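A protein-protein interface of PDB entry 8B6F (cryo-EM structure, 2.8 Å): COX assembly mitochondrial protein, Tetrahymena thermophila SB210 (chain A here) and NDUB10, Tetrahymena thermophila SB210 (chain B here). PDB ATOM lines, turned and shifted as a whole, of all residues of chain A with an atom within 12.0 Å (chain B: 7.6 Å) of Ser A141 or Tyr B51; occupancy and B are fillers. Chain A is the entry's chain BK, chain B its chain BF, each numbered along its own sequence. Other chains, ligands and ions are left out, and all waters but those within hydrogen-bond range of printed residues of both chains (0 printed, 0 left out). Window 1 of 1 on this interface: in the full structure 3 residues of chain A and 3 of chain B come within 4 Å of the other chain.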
ATOM      1  N   ALA A 136      -4.834  11.799  31.082  1.00  0.00           N
ATOM      2  CA  ALA A 136      -3.435  11.616  31.414  1.00  0.00           C
ATOM      3  C   ALA A 136      -2.698  10.979  30.239  1.00  0.00           C
ATOM      4  O   ALA A 136      -3.290  10.227  29.461  1.00  0.00           O
ATOM      5  CB  ALA A 136      -3.288  10.739  32.651  1.00  0.00           C
ATOM      6  N   PRO A 137      -1.409  11.264  30.084  1.00  0.00           N
ATOM      7  CA  PRO A 137      -0.654  10.642  28.993  1.00  0.00           C
ATOM      8  C   PRO A 137      -0.513   9.144  29.199  1.00  0.00           C
ATOM      9  O   PRO A 137      -0.467   8.647  30.326  1.00  0.00           O
ATOM     10  CB  PRO A 137       0.706  11.345  29.054  1.00  0.00           C
ATOM     11  CG  PRO A 137       0.834  11.788  30.465  1.00  0.00           C
ATOM     12  CD  PRO A 137      -0.555  12.124  30.923  1.00  0.00           C
ATOM     13  N   LYS A 138      -0.449   8.422  28.084  1.00  0.00           N
ATOM     14  CA  LYS A 138      -0.212   6.980  28.091  1.00  0.00           C
ATOM     15  C   LYS A 138       1.275   6.761  27.845  1.00  0.00           C
ATOM     16  O   LYS A 138       1.753   6.877  26.714  1.00  0.00           O
ATOM     17  CB  LYS A 138      -1.065   6.274  27.044  1.00  0.00           C
ATOM     18  CG  LYS A 138      -2.547   6.240  27.375  1.00  0.00           C
ATOM     19  CD  LYS A 138      -3.294   5.335  26.414  1.00  0.00           C
ATOM     20  CE  LYS A 138      -4.792   5.371  26.659  1.00  0.00           C
ATOM     21  NZ  LYS A 138      -5.149   4.850  28.007  1.00  0.00           N
ATOM     22  N   ASN A 139       2.005   6.445  28.908  1.00  0.00           N
ATOM     23  CA  ASN A 139       3.441   6.250  28.817  1.00  0.00           C
ATOM     24  C   ASN A 139       3.755   4.811  28.431  1.00  0.00           C
ATOM     25  O   ASN A 139       3.011   3.884  28.758  1.00  0.00           O
ATOM     26  CB  ASN A 139       4.116   6.593  30.145  1.00  0.00           C
ATOM     27  CG  ASN A 139       3.751   7.975  30.644  1.00  0.00           C
ATOM     28  OD1 ASN A 139       4.259   8.980  30.150  1.00  0.00           O
ATOM     29  ND2 ASN A 139       2.870   8.033  31.633  1.00  0.00           N
ATOM     30  N   LEU A 140       4.869   4.635  27.724  1.00  0.00           N
ATOM     31  CA  LEU A 140       5.323   3.316  27.290  1.00  0.00           C
ATOM     32  C   LEU A 140       4.242   2.626  26.456  1.00  0.00           C
ATOM     33  O   LEU A 140       3.703   1.580  26.818  1.00  0.00           O
ATOM     34  CB  LEU A 140       5.736   2.459  28.492  1.00  0.00           C
ATOM     35  CG  LEU A 140       7.089   2.787  29.136  1.00  0.00           C
ATOM     36  CD1 LEU A 140       7.173   4.235  29.582  1.00  0.00           C
ATOM     37  CD2 LEU A 140       7.358   1.866  30.311  1.00  0.00           C
ATOM     38  N   SER A 141       3.930   3.247  25.324  1.00  0.00           N
ATOM     39  CA  SER A 141       2.927   2.715  24.419  1.00  0.00           C
ATOM     40  C   SER A 141       3.486   1.510  23.666  1.00  0.00           C
ATOM     41  O   SER A 141       4.647   1.125  23.821  1.00  0.00           O
ATOM     42  CB  SER A 141       2.469   3.798  23.445  1.00  0.00           C
ATOM     43  OG  SER A 141       1.533   3.286  22.512  1.00  0.00           O
ATOM     44  N   PHE A 142       2.636   0.903  22.839  1.00  0.00           N
ATOM     45  CA  PHE A 142       3.015  -0.252  22.042  1.00  0.00           C
ATOM     46  C   PHE A 142       2.944  -0.015  20.542  1.00  0.00           C
ATOM     47  O   PHE A 142       3.626  -0.722  19.795  1.00  0.00           O
ATOM     48  CB  PHE A 142       2.127  -1.457  22.387  1.00  0.00           C
ATOM     49  CG  PHE A 142       0.665  -1.215  22.155  1.00  0.00           C
ATOM     50  CD1 PHE A 142       0.099  -1.447  20.914  1.00  0.00           C
ATOM     51  CD2 PHE A 142      -0.147  -0.761  23.181  1.00  0.00           C
ATOM     52  CE1 PHE A 142      -1.245  -1.229  20.697  1.00  0.00           C
ATOM     53  CE2 PHE A 142      -1.494  -0.540  22.971  1.00  0.00           C
ATOM     54  CZ  PHE A 142      -2.042  -0.774  21.727  1.00  0.00           C
ATOM     55  N   ALA A 143       2.149   0.945  20.083  1.00  0.00           N
ATOM     56  CA  ALA A 143       1.972   1.194  18.662  1.00  0.00           C
ATOM     57  C   ALA A 143       2.916   2.289  18.181  1.00  0.00           C
ATOM     58  O   ALA A 143       3.388   3.125  18.955  1.00  0.00           O
ATOM     59  CB  ALA A 143       0.525   1.581  18.361  1.00  0.00           C
ATOM     60  N   PHE A 144       3.189   2.268  16.880  1.00  0.00           N
ATOM     61  CA  PHE A 144       4.039   3.269  16.244  1.00  0.00           C
ATOM     62  C   PHE A 144       5.453   3.259  16.817  1.00  0.00           C
ATOM     63  O   PHE A 144       5.725   2.647  17.850  1.00  0.00           O
ATOM     64  CB  PHE A 144       3.423   4.662  16.396  1.00  0.00           C
ATOM     65  CG  PHE A 144       2.059   4.789  15.785  1.00  0.00           C
ATOM     66  CD1 PHE A 144       0.926   4.472  16.517  1.00  0.00           C
ATOM     67  CD2 PHE A 144       1.910   5.225  14.480  1.00  0.00           C
ATOM     68  CE1 PHE A 144      -0.332   4.588  15.957  1.00  0.00           C
ATOM     69  CE2 PHE A 144       0.656   5.342  13.913  1.00  0.00           C
ATOM     70  CZ  PHE A 144      -0.467   5.025  14.652  1.00  0.00           C
ATOM     71  OXT PHE A 144       6.363   3.864  16.249  1.00  0.00           O
ATOM     72  N   LEU B  48      11.795  -1.152  17.811  1.00  0.00           N
ATOM     73  CA  LEU B  48      11.096  -1.510  19.035  1.00  0.00           C
ATOM     74  C   LEU B  48      10.028  -0.476  19.374  1.00  0.00           C
ATOM     75  O   LEU B  48      10.116   0.691  18.986  1.00  0.00           O
ATOM     76  CB  LEU B  48      12.086  -1.626  20.193  1.00  0.00           C
ATOM     77  CG  LEU B  48      13.264  -2.578  19.977  1.00  0.00           C
ATOM     78  CD1 LEU B  48      14.198  -2.547  21.172  1.00  0.00           C
ATOM     79  CD2 LEU B  48      12.779  -3.990  19.713  1.00  0.00           C
ATOM     80  N   SER B  49       9.014  -0.921  20.113  1.00  0.00           N
ATOM     81  CA  SER B  49       7.969  -0.023  20.578  1.00  0.00           C
ATOM     82  C   SER B  49       8.513   0.880  21.683  1.00  0.00           C
ATOM     83  O   SER B  49       9.690   0.829  22.046  1.00  0.00           O
ATOM     84  CB  SER B  49       6.764  -0.820  21.068  1.00  0.00           C
ATOM     85  OG  SER B  49       7.107  -1.640  22.171  1.00  0.00           O
ATOM     86  N   SER B  50       7.635   1.719  22.234  1.00  0.00           N
ATOM     87  CA  SER B  50       8.054   2.620  23.301  1.00  0.00           C
ATOM     88  C   SER B  50       8.421   1.837  24.556  1.00  0.00           C
ATOM     89  O   SER B  50       9.465   2.081  25.169  1.00  0.00           O
ATOM     90  CB  SER B  50       6.948   3.631  23.600  1.00  0.00           C
ATOM     91  OG  SER B  50       7.360   4.554  24.592  1.00  0.00           O
ATOM     92  N   TYR B  51       7.567   0.894  24.954  1.00  0.00           N
ATOM     93  CA  TYR B  51       7.872   0.067  26.116  1.00  0.00           C
ATOM     94  C   TYR B  51       9.124  -0.768  25.881  1.00  0.00           C
ATOM     95  O   TYR B  51       9.993  -0.859  26.755  1.00  0.00           O
ATOM     96  CB  TYR B  51       6.678  -0.833  26.432  1.00  0.00           C
ATOM     97  CG  TYR B  51       6.866  -1.707  27.648  1.00  0.00           C
ATOM     98  CD1 TYR B  51       7.543  -2.914  27.551  1.00  0.00           C
ATOM     99  CD2 TYR B  51       6.351  -1.343  28.882  1.00  0.00           C
ATOM    100  CE1 TYR B  51       7.717  -3.723  28.645  1.00  0.00           C
ATOM    101  CE2 TYR B  51       6.520  -2.150  29.987  1.00  0.00           C
ATOM    102  CZ  TYR B  51       7.208  -3.339  29.859  1.00  0.00           C
ATOM    103  OH  TYR B  51       7.389  -4.160  30.941  1.00  0.00           O
ATOM    104  N   ASP B  52       9.234  -1.381  24.701  1.00  0.00           N
ATOM    105  CA  ASP B  52      10.391  -2.216  24.402  1.00  0.00           C
ATOM    106  C   ASP B  52      11.679  -1.407  24.397  1.00  0.00           C
ATOM    107  O   ASP B  52      12.720  -1.884  24.863  1.00  0.00           O
ATOM    108  CB  ASP B  52      10.194  -2.927  23.064  1.00  0.00           C
ATOM    109  CG  ASP B  52       9.159  -4.028  23.139  1.00  0.00           C
ATOM    110  OD1 ASP B  52       8.980  -4.600  24.233  1.00  0.00           O
ATOM    111  OD2 ASP B  52       8.525  -4.326  22.106  1.00  0.00           O
ATOM    112  N   TYR B  53      11.637  -0.183  23.871  1.00  0.00           N
ATOM    113  CA  TYR B  53      12.847   0.629  23.860  1.00  0.00           C
ATOM    114  C   TYR B  53      13.170   1.188  25.238  1.00  0.00           C
ATOM    115  O   TYR B  53      14.345   1.414  25.547  1.00  0.00           O
ATOM    116  CB  TYR B  53      12.736   1.774  22.858  1.00  0.00           C
ATOM    117  CG  TYR B  53      14.023   2.555  22.774  1.00  0.00           C
ATOM    118  CD1 TYR B  53      15.067   2.123  21.967  1.00  0.00           C
ATOM    119  CD2 TYR B  53      14.213   3.698  23.537  1.00  0.00           C
ATOM    120  CE1 TYR B  53      16.254   2.822  21.905  1.00  0.00           C
ATOM    121  CE2 TYR B  53      15.396   4.402  23.481  1.00  0.00           C
ATOM    122  CZ  TYR B  53      16.412   3.960  22.664  1.00  0.00           C
ATOM    123  OH  TYR B  53      17.591   4.660  22.606  1.00  0.00           O
ATOM    124  N   PHE B  54      12.163   1.422  26.080  1.00  0.00           N
ATOM    125  CA  PHE B  54      12.463   1.781  27.460  1.00  0.00           C
ATOM    126  C   PHE B  54      13.190   0.638  28.156  1.00  0.00           C
ATOM    127  O   PHE B  54      14.164   0.862  28.883  1.00  0.00           O
ATOM    128  CB  PHE B  54      11.179   2.142  28.205  1.00  0.00           C
ATOM    129  CG  PHE B  54      11.413   2.689  29.584  1.00  0.00           C
ATOM    130  CD1 PHE B  54      11.541   1.841  30.667  1.00  0.00           C
ATOM    131  CD2 PHE B  54      11.497   4.053  29.797  1.00  0.00           C
ATOM    132  CE1 PHE B  54      11.754   2.338  31.938  1.00  0.00           C
ATOM    133  CE2 PHE B  54      11.710   4.559  31.064  1.00  0.00           C
ATOM    134  CZ  PHE B  54      11.838   3.700  32.136  1.00  0.00           C
ATOM    135  N   ALA B  55      12.726  -0.596  27.948  1.00  0.00           N
ATOM    136  CA  ALA B  55      13.432  -1.750  28.493  1.00  0.00           C
ATOM    137  C   ALA B  55      14.839  -1.848  27.916  1.00  0.00           C
ATOM    138  O   ALA B  55      15.797  -2.149  28.636  1.00  0.00           O
ATOM    139  CB  ALA B  55      12.644  -3.028  28.207  1.00  0.00           C
ATOM    140  N   PHE B  56      14.977  -1.597  26.611  1.00  0.00           N
ATOM    141  CA  PHE B  56      16.287  -1.631  25.967  1.00  0.00           C
ATOM    142  C   PHE B  56      17.217  -0.586  26.566  1.00  0.00           C
ATOM    143  O   PHE B  56      18.392  -0.865  26.828  1.00  0.00           O
ATOM    144  CB  PHE B  56      16.122  -1.410  24.462  1.00  0.00           C
ATOM    145  CG  PHE B  56      17.414  -1.410  23.695  1.00  0.00           C
ATOM    146  CD1 PHE B  56      18.170  -0.255  23.577  1.00  0.00           C
ATOM    147  CD2 PHE B  56      17.855  -2.558  23.061  1.00  0.00           C
ATOM    148  CE1 PHE B  56      19.351  -0.254  22.861  1.00  0.00           C
ATOM    149  CE2 PHE B  56      19.034  -2.562  22.346  1.00  0.00           C
ATOM    150  CZ  PHE B  56      19.781  -1.408  22.245  1.00  0.00           C
ATOM    151  N   LYS B  57      16.706   0.623  26.793  1.00  0.00           N
ATOM    152  CA  LYS B  57      17.520   1.676  27.389  1.00  0.00           C
ATOM    153  C   LYS B  57      17.964   1.301  28.795  1.00  0.00           C
ATOM    154  O   LYS B  57      19.129   1.493  29.157  1.00  0.00           O
ATOM    155  CB  LYS B  57      16.726   2.983  27.405  1.00  0.00           C
ATOM    156  CG  LYS B  57      17.399   4.133  28.139  1.00  0.00           C
ATOM    157  CD  LYS B  57      16.430   5.280  28.375  1.00  0.00           C
ATOM    158  CE  LYS B  57      15.407   4.959  29.457  1.00  0.00           C
ATOM    159  NZ  LYS B  57      16.040   4.711  30.782  1.00  0.00           N
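The backbone NH of Tyr B51 is in hydrogen-bond range of the backbone carbonyl oxygen of Ser A141. O of Ser A141 lies close to N of Ser B50, at 3.4 Å.
The side-chain carboxylate (OD2) of Asp B52 lies within hydrogen-bond range of the side-chain hydroxyl (OG) of Ser B49, 3.0 Å away. The side-chain hydroxyl (OG) of Ser A141 sits at hydrogen-bond distance from the backbone NH (N) of Ala A143, at 3.4 Å.
Ser B50 touches Leu A140 (OG to CA, 3.6 Å). Leu A140 touches Tyr B51. Ser B49 touches Ser A141 (CB to O, 3.98 Å). O of Phe A142 touches CB of Ser B49 (3.4 Å).
Of the printed residues of chain B, Ser A141 touches Ser B49 (3.98 Å), Ser B50 (3.4 Å) and Tyr B51 (3.1 Å). Tyr B51 touches two residues of chain A. Ser B50 touches just these residues of chain A: Leu A140 (3.6 Å) and Ser A141 (3.4 Å). No residue of chain A comes within 4 Å of Phe B54. Of the printed residues of chain B, Leu A140 touches Ser B50 (3.6 Å) and Tyr B51 (3.7 Å). Of the printed residues of chain A, Ser B49 touches Ser A141 (3.98 Å) and Phe A142 (3.4 Å). Of the printed residues of chain B, Phe A142 touches Ser B49. Lys A138 touches none of the printed residues of chain B. The nearest printed residue of chain B that does not touch Ser A141 is Asp B52 (5.3 Å). The nearest printed residue of chain A that does not touch Ser B49 is Phe A144 (4.4 Å).
Hydrophobic or aromatic side chains of chain A within 4 Å of the printed part of chain B: Leu A140. Printed residues of chain B that touch a printed residue of chain A: Ser B49, Ser B50 and Tyr B51. Hydrophobic or aromatic side chains of chain B that line the printed part of chain A: Tyr B51. Among the printed residues, 6 pairs touch across the chains. Among the printed residues, no Asp or Glu carboxylate lies within 4 Å of a Lys or Arg side-chain nitrogen of the other chain.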
